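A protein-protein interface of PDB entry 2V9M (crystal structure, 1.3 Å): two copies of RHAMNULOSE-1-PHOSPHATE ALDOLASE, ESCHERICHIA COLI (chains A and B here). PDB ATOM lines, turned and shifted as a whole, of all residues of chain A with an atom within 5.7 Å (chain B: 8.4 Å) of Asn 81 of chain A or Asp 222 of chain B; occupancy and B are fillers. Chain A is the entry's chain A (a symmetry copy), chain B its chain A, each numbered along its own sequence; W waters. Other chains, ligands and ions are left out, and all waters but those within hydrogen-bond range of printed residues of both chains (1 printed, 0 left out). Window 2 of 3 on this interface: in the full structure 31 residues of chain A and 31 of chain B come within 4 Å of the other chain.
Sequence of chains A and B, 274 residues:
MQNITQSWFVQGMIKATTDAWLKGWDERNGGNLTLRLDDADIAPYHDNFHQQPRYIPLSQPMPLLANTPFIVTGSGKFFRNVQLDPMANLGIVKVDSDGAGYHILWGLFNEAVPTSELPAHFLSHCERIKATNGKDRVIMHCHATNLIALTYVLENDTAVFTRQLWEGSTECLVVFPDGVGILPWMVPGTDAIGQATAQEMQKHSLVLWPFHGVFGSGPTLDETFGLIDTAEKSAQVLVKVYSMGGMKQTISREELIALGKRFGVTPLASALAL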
ATOM      1  N   PHE A  78      -7.110  10.914  23.328  1.00  0.00           N
ATOM      2  CA  PHE A  78      -7.291  12.339  23.498  1.00  0.00           C
ATOM      3  C   PHE A  78      -6.999  13.091  22.201  1.00  0.00           C
ATOM      4  O   PHE A  78      -5.932  12.921  21.605  1.00  0.00           O
ATOM      5  CB  PHE A  78      -6.299  12.838  24.551  1.00  0.00           C
ATOM      6  CG  PHE A  78      -6.580  12.516  25.997  1.00  0.00           C
ATOM      7  CD1 PHE A  78      -7.360  11.476  26.401  1.00  0.00           C
ATOM      8  CD2 PHE A  78      -6.034  13.333  26.970  1.00  0.00           C
ATOM      9  CE1 PHE A  78      -7.571  11.253  27.759  1.00  0.00           C
ATOM     10  CE2 PHE A  78      -6.203  13.056  28.300  1.00  0.00           C
ATOM     11  CZ  PHE A  78      -6.947  12.024  28.726  1.00  0.00           C
ATOM     12  N   PHE A  79      -7.939  13.955  21.776  1.00  0.00           N
ATOM     13  CA  PHE A  79      -7.690  14.780  20.604  1.00  0.00           C
ATOM     14  C   PHE A  79      -6.383  15.532  20.732  1.00  0.00           C
ATOM     15  O   PHE A  79      -5.675  15.717  19.739  1.00  0.00           O
ATOM     16  CB  PHE A  79      -8.806  15.800  20.359  1.00  0.00           C
ATOM     17  CG  PHE A  79     -10.011  15.303  19.589  1.00  0.00           C
ATOM     18  CD1 PHE A  79     -10.372  13.969  19.524  1.00  0.00           C
ATOM     19  CD2 PHE A  79     -10.793  16.207  18.907  1.00  0.00           C
ATOM     20  CE1 PHE A  79     -11.472  13.588  18.787  1.00  0.00           C
ATOM     21  CE2 PHE A  79     -11.910  15.851  18.210  1.00  0.00           C
ATOM     22  CZ  PHE A  79     -12.253  14.525  18.162  1.00  0.00           C
ATOM     23  N   ARG A  80      -6.055  15.993  21.927  1.00  0.00           N
ATOM     24  CA  ARG A  80      -4.811  16.762  22.149  1.00  0.00           C
ATOM     25  C   ARG A  80      -3.578  15.989  21.717  1.00  0.00           C
ATOM     26  O   ARG A  80      -2.563  16.616  21.364  1.00  0.00           O
ATOM     27  CB  ARG A  80      -4.726  17.116  23.641  1.00  0.00           C
ATOM     28  CG  ARG A  80      -3.565  18.097  23.967  1.00  0.00           C
ATOM     29  CD  ARG A  80      -2.313  17.434  24.499  1.00  0.00           C
ATOM     30  NE  ARG A  80      -1.268  18.424  24.679  1.00  0.00           N
ATOM     31  CZ  ARG A  80      -0.480  18.878  23.753  1.00  0.00           C
ATOM     32  NH1 ARG A  80      -0.465  18.393  22.500  1.00  0.00           N
ATOM     33  NH2 ARG A  80       0.369  19.821  24.073  1.00  0.00           N
ATOM     34  N   ASN A  81      -3.602  14.667  21.796  1.00  0.00           N
ATOM     35  CA  ASN A  81      -2.425  13.849  21.563  1.00  0.00           C
ATOM     36  C   ASN A  81      -2.251  13.414  20.112  1.00  0.00           C
ATOM     37  O   ASN A  81      -1.203  12.855  19.776  1.00  0.00           O
ATOM     38  CB  ASN A  81      -2.447  12.619  22.469  1.00  0.00           C
ATOM     39  CG  ASN A  81      -2.199  12.945  23.924  1.00  0.00           C
ATOM     40  OD1 ASN A  81      -1.610  13.962  24.223  1.00  0.00           O
ATOM     41  ND2 ASN A  81      -2.670  12.007  24.751  1.00  0.00           N
ATOM     42  N   VAL A  82      -3.280  13.615  19.270  1.00  0.00           N
ATOM     43  CA  VAL A  82      -3.200  13.098  17.894  1.00  0.00           C
ATOM     44  C   VAL A  82      -1.953  13.649  17.201  1.00  0.00           C
ATOM     45  O   VAL A  82      -1.224  12.921  16.529  1.00  0.00           O
ATOM     46  CB  VAL A  82      -4.500  13.377  17.129  1.00  0.00           C
ATOM     47  CG1 VAL A  82      -4.393  12.967  15.676  1.00  0.00           C
ATOM     48  CG2 VAL A  82      -5.656  12.604  17.759  1.00  0.00           C
ATOM     49  N   GLN A  83      -1.686  14.951  17.390  1.00  0.00           N
ATOM     50  CA  GLN A  83      -0.516  15.563  16.755  1.00  0.00           C
ATOM     51  C   GLN A  83       0.817  15.021  17.230  1.00  0.00           C
ATOM     52  O   GLN A  83       1.794  15.142  16.505  1.00  0.00           O
ATOM     53  CB  GLN A  83      -0.565  17.082  17.003  1.00  0.00           C
ATOM     54  CG  GLN A  83      -0.439  17.479  18.455  1.00  0.00           C
ATOM     55  CD  GLN A  83      -0.732  18.959  18.671  1.00  0.00           C
ATOM     56  OE1 GLN A  83      -0.137  19.820  18.023  1.00  0.00           O
ATOM     57  NE2 GLN A  83      -1.641  19.183  19.613  1.00  0.00           N
ATOM     58  N   LEU A  84       0.842  14.499  18.459  1.00  0.00           N
ATOM     59  CA  LEU A  84       2.082  13.991  19.037  1.00  0.00           C
ATOM     60  C   LEU A  84       2.396  12.583  18.575  1.00  0.00           C
ATOM     61  O   LEU A  84       3.557  12.203  18.550  1.00  0.00           O
ATOM     62  CB  LEU A  84       1.978  14.008  20.571  1.00  0.00           C
ATOM     63  CG  LEU A  84       1.754  15.351  21.234  1.00  0.00           C
ATOM     64  CD1 LEU A  84       1.629  15.201  22.739  1.00  0.00           C
ATOM     65  CD2 LEU A  84       2.895  16.322  20.914  1.00  0.00           C
ATOM     66  N   ASP A  85       1.394  11.785  18.271  1.00  0.00           N
ATOM     67  CA  ASP A  85       1.562  10.363  17.941  1.00  0.00           C
ATOM     68  C   ASP A  85       0.343   9.907  17.178  1.00  0.00           C
ATOM     69  O   ASP A  85      -0.579   9.265  17.719  1.00  0.00           O
ATOM     70  CB  ASP A  85       1.754   9.538  19.206  1.00  0.00           C
ATOM     71  CG  ASP A  85       2.294   8.137  18.962  1.00  0.00           C
ATOM     72  OD1 ASP A  85       2.844   7.495  19.919  1.00  0.00           O
ATOM     73  OD2 ASP A  85       2.176   7.659  17.794  1.00  0.00           O
ATOM     74  N   PRO A  86       0.304  10.242  15.876  1.00  0.00           N
ATOM     75  CA  PRO A  86      -0.904   9.881  15.102  1.00  0.00           C
ATOM     76  C   PRO A  86      -1.106   8.381  15.035  1.00  0.00           C
ATOM     77  O   PRO A  86      -2.251   7.925  15.067  1.00  0.00           O
ATOM     78  CB  PRO A  86      -0.665  10.525  13.751  1.00  0.00           C
ATOM     79  CG  PRO A  86       0.772  10.857  13.704  1.00  0.00           C
ATOM     80  CD  PRO A  86       1.228  11.093  15.131  1.00  0.00           C
ATOM     81  N   ASN A  89      -2.959   7.114  18.123  1.00  0.00           N
ATOM     82  CA  ASN A  89      -4.254   7.718  18.434  1.00  0.00           C
ATOM     83  C   ASN A  89      -5.268   7.637  17.299  1.00  0.00           C
ATOM     84  O   ASN A  89      -6.440   7.917  17.577  1.00  0.00           O
ATOM     85  CB  ASN A  89      -4.042   9.164  18.876  1.00  0.00           C
ATOM     86  CG  ASN A  89      -3.287   9.239  20.171  1.00  0.00           C
ATOM     87  OD1 ASN A  89      -3.870   8.854  21.191  1.00  0.00           O
ATOM     88  ND2 ASN A  89      -2.065   9.680  20.173  1.00  0.00           N
ATOM     89  N   TRP B   8      10.760  10.539  28.797  1.00  0.00           N
ATOM     90  CA  TRP B   8       9.283  10.599  28.725  1.00  0.00           C
ATOM     91  C   TRP B   8       8.725  11.475  29.842  1.00  0.00           C
ATOM     92  O   TRP B   8       7.747  12.198  29.633  1.00  0.00           O
ATOM     93  CB  TRP B   8       8.626   9.210  28.724  1.00  0.00           C
ATOM     94  CG  TRP B   8       8.676   8.465  30.027  1.00  0.00           C
ATOM     95  CD1 TRP B   8       9.558   7.514  30.453  1.00  0.00           C
ATOM     96  CD2 TRP B   8       7.745   8.614  31.124  1.00  0.00           C
ATOM     97  NE1 TRP B   8       9.265   7.087  31.708  1.00  0.00           N
ATOM     98  CE2 TRP B   8       8.129   7.751  32.148  1.00  0.00           C
ATOM     99  CE3 TRP B   8       6.627   9.404  31.319  1.00  0.00           C
ATOM    100  CZ2 TRP B   8       7.446   7.654  33.334  1.00  0.00           C
ATOM    101  CZ3 TRP B   8       5.934   9.333  32.486  1.00  0.00           C
ATOM    102  CH2 TRP B   8       6.343   8.454  33.506  1.00  0.00           C
ATOM    103  N   GLY B  12       6.758  14.854  29.593  1.00  0.00           N
ATOM    104  CA  GLY B  12       5.377  14.839  30.060  1.00  0.00           C
ATOM    105  C   GLY B  12       5.099  15.976  31.039  1.00  0.00           C
ATOM    106  O   GLY B  12       4.027  16.607  30.982  1.00  0.00           O
ATOM    107  N   LYS B  15       4.674  19.037  28.996  1.00  0.00           N
ATOM    108  CA  LYS B  15       3.414  19.111  28.284  1.00  0.00           C
ATOM    109  C   LYS B  15       2.315  19.523  29.230  1.00  0.00           C
ATOM    110  O   LYS B  15       1.481  20.371  28.896  1.00  0.00           O
ATOM    111  CB  LYS B  15       3.110  17.736  27.654  1.00  0.00           C
ATOM    112  CG  LYS B  15       1.859  17.751  26.788  1.00  0.00           C
ATOM    113  CD  LYS B  15       1.517  16.380  26.267  1.00  0.00           C
ATOM    114  CE  LYS B  15       0.240  15.823  26.614  1.00  0.00           C
ATOM    115  NZ  LYS B  15      -0.030  14.437  26.386  1.00  0.00           N
ATOM    116  N   ALA B  16       2.256  18.887  30.413  1.00  0.00           N
ATOM    117  CA  ALA B  16       1.144  19.150  31.335  1.00  0.00           C
ATOM    118  C   ALA B  16       1.163  20.581  31.868  1.00  0.00           C
ATOM    119  O   ALA B  16       0.123  21.248  31.942  1.00  0.00           O
ATOM    120  CB  ALA B  16       1.161  18.143  32.482  1.00  0.00           C
ATOM    121  N   ASP B  19       0.312  22.997  28.964  1.00  0.00           N
ATOM    122  CA  ASP B  19      -1.097  22.953  28.649  1.00  0.00           C
ATOM    123  C   ASP B  19      -1.901  23.688  29.711  1.00  0.00           C
ATOM    124  O   ASP B  19      -2.840  24.417  29.375  1.00  0.00           O
ATOM    125  CB  ASP B  19      -1.574  21.522  28.531  1.00  0.00           C
ATOM    126  CG  ASP B  19      -1.126  20.770  27.304  1.00  0.00           C
ATOM    127  OD1 ASP B  19      -0.575  21.397  26.372  1.00  0.00           O
ATOM    128  OD2 ASP B  19      -1.321  19.525  27.255  1.00  0.00           O
ATOM    129  N   LEU B  33       2.660  20.332  40.628  1.00  0.00           N
ATOM    130  CA  LEU B  33       2.495  19.091  39.921  1.00  0.00           C
ATOM    131  C   LEU B  33       3.587  18.114  40.390  1.00  0.00           C
ATOM    132  O   LEU B  33       4.780  18.450  40.300  1.00  0.00           O
ATOM    133  CB  LEU B  33       2.556  19.281  38.407  1.00  0.00           C
ATOM    134  CG  LEU B  33       2.357  18.024  37.553  1.00  0.00           C
ATOM    135  CD1 LEU B  33       1.025  17.393  37.766  1.00  0.00           C
ATOM    136  CD2 LEU B  33       2.567  18.391  36.077  1.00  0.00           C
ATOM    137  N   LEU B  35       4.708  13.875  40.158  1.00  0.00           N
ATOM    138  CA  LEU B  35       4.562  12.592  39.462  1.00  0.00           C
ATOM    139  C   LEU B  35       5.459  11.563  40.080  1.00  0.00           C
ATOM    140  O   LEU B  35       6.681  11.746  40.105  1.00  0.00           O
ATOM    141  CB  LEU B  35       4.894  12.777  37.981  1.00  0.00           C
ATOM    142  CG  LEU B  35       5.102  11.505  37.144  1.00  0.00           C
ATOM    143  CD1 LEU B  35       3.797  10.684  37.057  1.00  0.00           C
ATOM    144  CD2 LEU B  35       5.577  11.844  35.739  1.00  0.00           C
ATOM    145  N   VAL B 138      -0.080  10.707  40.335  1.00  0.00           N
ATOM    146  CA  VAL B 138       0.018  12.108  40.045  1.00  0.00           C
ATOM    147  C   VAL B 138      -0.871  12.898  41.046  1.00  0.00           C
ATOM    148  O   VAL B 138      -2.003  12.496  41.272  1.00  0.00           O
ATOM    149  CB  VAL B 138      -0.421  12.438  38.620  1.00  0.00           C
ATOM    150  CG1 VAL B 138      -0.306  13.939  38.340  1.00  0.00           C
ATOM    151  CG2 VAL B 138       0.366  11.598  37.633  1.00  0.00           C
ATOM    152  N   MET B 140      -1.985  16.973  41.099  1.00  0.00           N
ATOM    153  CA  MET B 140      -1.930  18.217  40.363  1.00  0.00           C
ATOM    154  C   MET B 140      -2.811  19.273  41.031  1.00  0.00           C
ATOM    155  O   MET B 140      -3.996  19.023  41.272  1.00  0.00           O
ATOM    156  CB  MET B 140      -2.419  18.023  38.932  1.00  0.00           C
ATOM    157  CG  MET B 140      -2.375  19.274  38.085  1.00  0.00           C
ATOM    158  SD  MET B 140      -2.653  18.945  36.362  1.00  0.00           S
ATOM    159  CE  MET B 140      -3.046  20.625  35.814  1.00  0.00           C
ATOM    160  N   GLY B 218      -4.534  11.013  39.769  1.00  0.00           N
ATOM    161  CA  GLY B 218      -4.787  10.018  38.742  1.00  0.00           C
ATOM    162  C   GLY B 218      -3.556   9.189  38.424  1.00  0.00           C
ATOM    163  O   GLY B 218      -2.477   9.415  38.992  1.00  0.00           O
ATOM    164  N   PRO B 219      -3.700   8.200  37.555  1.00  0.00           N
ATOM    165  CA  PRO B 219      -2.614   7.251  37.288  1.00  0.00           C
ATOM    166  C   PRO B 219      -1.512   7.759  36.335  1.00  0.00           C
ATOM    167  O   PRO B 219      -0.405   7.250  36.381  1.00  0.00           O
ATOM    168  CB  PRO B 219      -3.300   6.065  36.620  1.00  0.00           C
ATOM    169  CG  PRO B 219      -4.660   6.490  36.281  1.00  0.00           C
ATOM    170  CD  PRO B 219      -4.980   7.735  37.010  1.00  0.00           C
ATOM    171  N   THR B 220      -1.827   8.724  35.494  1.00  0.00           N
ATOM    172  CA  THR B 220      -0.917   9.284  34.528  1.00  0.00           C
ATOM    173  C   THR B 220      -1.125  10.790  34.481  1.00  0.00           C
ATOM    174  O   THR B 220      -2.184  11.311  34.901  1.00  0.00           O
ATOM    175  CB  THR B 220      -1.103   8.717  33.101  1.00  0.00           C
ATOM    176  OG1 THR B 220      -2.373   9.159  32.604  1.00  0.00           O
ATOM    177  CG2 THR B 220      -1.021   7.215  33.056  1.00  0.00           C
ATOM    178  N   LEU B 221      -0.163  11.484  33.930  1.00  0.00           N
ATOM    179  CA  LEU B 221      -0.305  12.927  33.700  1.00  0.00           C
ATOM    180  C   LEU B 221      -1.531  13.227  32.868  1.00  0.00           C
ATOM    181  O   LEU B 221      -2.354  14.110  33.234  1.00  0.00           O
ATOM    182  CB  LEU B 221       0.962  13.519  33.044  1.00  0.00           C
ATOM    183  CG  LEU B 221       2.198  13.537  33.960  1.00  0.00           C
ATOM    184  CD1 LEU B 221       3.436  13.888  33.140  1.00  0.00           C
ATOM    185  CD2 LEU B 221       2.027  14.529  35.081  1.00  0.00           C
ATOM    186  N   ASP B 222      -1.703  12.543  31.721  1.00  0.00           N
ATOM    187  CA  ASP B 222      -2.870  12.828  30.892  1.00  0.00           C
ATOM    188  C   ASP B 222      -4.192  12.549  31.602  1.00  0.00           C
ATOM    189  O   ASP B 222      -5.148  13.312  31.454  1.00  0.00           O
ATOM    190  CB  ASP B 222      -2.822  12.027  29.622  1.00  0.00           C
ATOM    191  CG  ASP B 222      -1.943  12.533  28.522  1.00  0.00           C
ATOM    192  OD1 ASP B 222      -1.738  11.772  27.529  1.00  0.00           O
ATOM    193  OD2 ASP B 222      -1.441  13.663  28.628  1.00  0.00           O
ATOM    194  N   GLU B 223      -4.267  11.449  32.344  1.00  0.00           N
ATOM    195  CA  GLU B 223      -5.568  11.150  32.971  1.00  0.00           C
ATOM    196  C   GLU B 223      -5.867  12.172  34.054  1.00  0.00           C
ATOM    197  O   GLU B 223      -7.022  12.546  34.276  1.00  0.00           O
ATOM    198  CB  GLU B 223      -5.558   9.712  33.474  1.00  0.00           C
ATOM    199  CG  GLU B 223      -5.582   8.639  32.383  1.00  0.00           C
ATOM    200  CD  GLU B 223      -5.447   7.237  32.966  1.00  0.00           C
ATOM    201  OE1 GLU B 223      -6.361   6.604  33.545  1.00  0.00           O
ATOM    202  OE2 GLU B 223      -4.322   6.741  32.839  1.00  0.00           O
ATOM    203  N   THR B 224      -4.844  12.634  34.779  1.00  0.00           N
ATOM    204  CA  THR B 224      -5.046  13.593  35.870  1.00  0.00           C
ATOM    205  C   THR B 224      -5.423  14.945  35.318  1.00  0.00           C
ATOM    206  O   THR B 224      -6.366  15.600  35.766  1.00  0.00           O
ATOM    207  CB  THR B 224      -3.812  13.660  36.754  1.00  0.00           C
ATOM    208  OG1 THR B 224      -3.455  12.352  37.202  1.00  0.00           O
ATOM    209  CG2 THR B 224      -4.113  14.485  37.994  1.00  0.00           C
ATOM    210  N   PHE B 225      -4.664  15.400  34.291  1.00  0.00           N
ATOM    211  CA  PHE B 225      -5.021  16.635  33.594  1.00  0.00           C
ATOM    212  C   PHE B 225      -6.434  16.487  33.055  1.00  0.00           C
ATOM    213  O   PHE B 225      -7.207  17.455  33.196  1.00  0.00           O
ATOM    214  CB  PHE B 225      -4.001  16.895  32.472  1.00  0.00           C
ATOM    215  CG  PHE B 225      -4.198  18.230  31.783  1.00  0.00           C
ATOM    216  CD1 PHE B 225      -3.393  19.298  32.093  1.00  0.00           C
ATOM    217  CD2 PHE B 225      -5.190  18.398  30.818  1.00  0.00           C
ATOM    218  CE1 PHE B 225      -3.609  20.530  31.483  1.00  0.00           C
ATOM    219  CE2 PHE B 225      -5.441  19.618  30.242  1.00  0.00           C
ATOM    220  CZ  PHE B 225      -4.632  20.672  30.585  1.00  0.00           C
ATOM    221  N   GLY B 226      -6.743  15.380  32.386  1.00  0.00           N
ATOM    222  CA  GLY B 226      -8.061  15.216  31.803  1.00  0.00           C
ATOM    223  C   GLY B 226      -9.184  15.214  32.796  1.00  0.00           C
ATOM    224  O   GLY B 226     -10.292  15.658  32.478  1.00  0.00           O
ATOM    225  N   LEU B 227      -8.937  14.726  33.995  1.00  0.00           N
ATOM    226  CA  LEU B 227      -9.900  14.739  35.092  1.00  0.00           C
ATOM    227  C   LEU B 227     -10.251  16.193  35.457  1.00  0.00           C
ATOM    228  O   LEU B 227     -11.415  16.603  35.556  1.00  0.00           O
ATOM    229  CB  LEU B 227      -9.304  13.981  36.268  1.00  0.00           C
ATOM    230  CG  LEU B 227     -10.022  14.076  37.613  1.00  0.00           C
ATOM    231  CD1 LEU B 227     -11.413  13.437  37.494  1.00  0.00           C
ATOM    232  CD2 LEU B 227      -9.181  13.418  38.708  1.00  0.00           C
ATOM    233  N   ILE B 228      -9.185  16.963  35.723  1.00  0.00           N
ATOM    234  CA  ILE B 228      -9.350  18.381  36.038  1.00  0.00           C
ATOM    235  C   ILE B 228     -10.029  19.099  34.882  1.00  0.00           C
ATOM    236  O   ILE B 228     -10.958  19.887  35.104  1.00  0.00           O
ATOM    237  CB  ILE B 228      -8.005  19.030  36.448  1.00  0.00           C
ATOM    238  CG1 ILE B 228      -7.526  18.481  37.776  1.00  0.00           C
ATOM    239  CG2 ILE B 228      -8.095  20.534  36.464  1.00  0.00           C
ATOM    240  CD1 ILE B 228      -6.101  18.838  38.123  1.00  0.00           C
ATOM    241  N   ASP B 229      -9.589  18.842  33.657  1.00  0.00           N
ATOM    242  CA  ASP B 229     -10.152  19.516  32.495  1.00  0.00           C
ATOM    243  C   ASP B 229     -11.641  19.216  32.334  1.00  0.00           C
ATOM    244  O   ASP B 229     -12.452  20.066  31.924  1.00  0.00           O
ATOM    245  CB  ASP B 229      -9.373  19.126  31.242  1.00  0.00           C
ATOM    246  CG  ASP B 229      -9.462  20.096  30.084  1.00  0.00           C
ATOM    247  OD1 ASP B 229      -9.712  21.291  30.308  1.00  0.00           O
ATOM    248  OD2 ASP B 229      -9.178  19.625  28.948  1.00  0.00           O
ATOM    249  N   THR B 230     -12.042  17.978  32.671  1.00  0.00           N
ATOM    250  CA  THR B 230     -13.446  17.610  32.580  1.00  0.00           C
ATOM    251  C   THR B 230     -14.284  18.411  33.591  1.00  0.00           C
ATOM    252  O   THR B 230     -15.328  18.969  33.258  1.00  0.00           O
ATOM    253  CB  THR B 230     -13.613  16.110  32.835  1.00  0.00           C
ATOM    254  OG1 THR B 230     -12.871  15.433  31.825  1.00  0.00           O
ATOM    255  CG2 THR B 230     -15.039  15.652  32.774  1.00  0.00           C
HETATM  256  O   HOH W   1       2.119  21.910  25.572  1.00  0.00           O
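Water W1 bridges the side-chain carboxylate (OD1) of Asp 19 of chain B (2.9 Å) and the guanidinium group (NH2) of Arg 80 of chain A (3.1 Å).
No position is printed for both chains. Of the 6 pairs that touch across the chains among the printed residues, none has its exchanged pair printed and touching as well.
NZ of Lys 15 of chain B lies within hydrogen-bond range of OD1 of Asn 81 of chain A, at 2.7 Å. OD2 of Asp 19 of chain B lies within salt-bridge range of NE of Arg 80 of chain A, 2.8 Å away. The side-chain amide nitrogen of Asn 81 of chain A lies within hydrogen-bond range of the side-chain carboxylate of Asp 222 of chain B, 2.9 Å away.
CE2 of Phe 78 of chain A touches O of Asp 222 of chain B (3.3 Å). Lys 15 of chain B touches Arg 80 of chain A. Lys 15 of chain B touches Leu 84 of chain A (CD to CD1, 3.7 Å).
ND2 of Asn 89 of chain A sits at hydrogen-bond distance from O of Asn 81 of chain A, 3.3 Å away. The side-chain amino group of Lys 15 of chain B lies within salt-bridge range of the side-chain carboxylate of Asp 222 of chain B, at 2.8 Å. NH1 of Arg 80 of chain A lies close to NE2 of Gln 83 of chain A (3.2 Å).
Of chain B, only Lys 15 (2.7 Å) and Asp 222 (2.9 Å) come within 4 Å of Asn 81 of chain A. Of the printed residues of chain B, Leu 84 of chain A touches Lys 15 (3.7 Å). Of the printed residues of chain A, Lys 15 of chain B touches Arg 80, Asn 81 and Leu 84. Leu 35 of chain B touches none of the printed residues of chain A. Printed residues of chain A within 4 Å of Asp 222 of chain B: Phe 78 (3.3 Å) and Asn 81 (2.9 Å). Leu 227 of chain B touches none of the printed residues of chain A.
Of the 10 printed residues of chain A, 4 touch a printed residue of chain B. Printed residues of chain A that touch a printed residue of chain B: Phe 78, Arg 80, Asn 81 and Leu 84. Hydrophobic or aromatic side chains of chain A within 4 Å of the printed part of chain B: Phe 78 and Leu 84. Of the 22 printed residues of chain B, 3 touch a printed residue of chain A. Among the printed residues, 6 pairs touch across the chains. Among the printed residues, Asp or Glu carboxylates within 4 Å of a Lys or Arg side-chain nitrogen of the other chain: Arg 80 of chain A with Asp 19 of chain B (2.8 Å).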
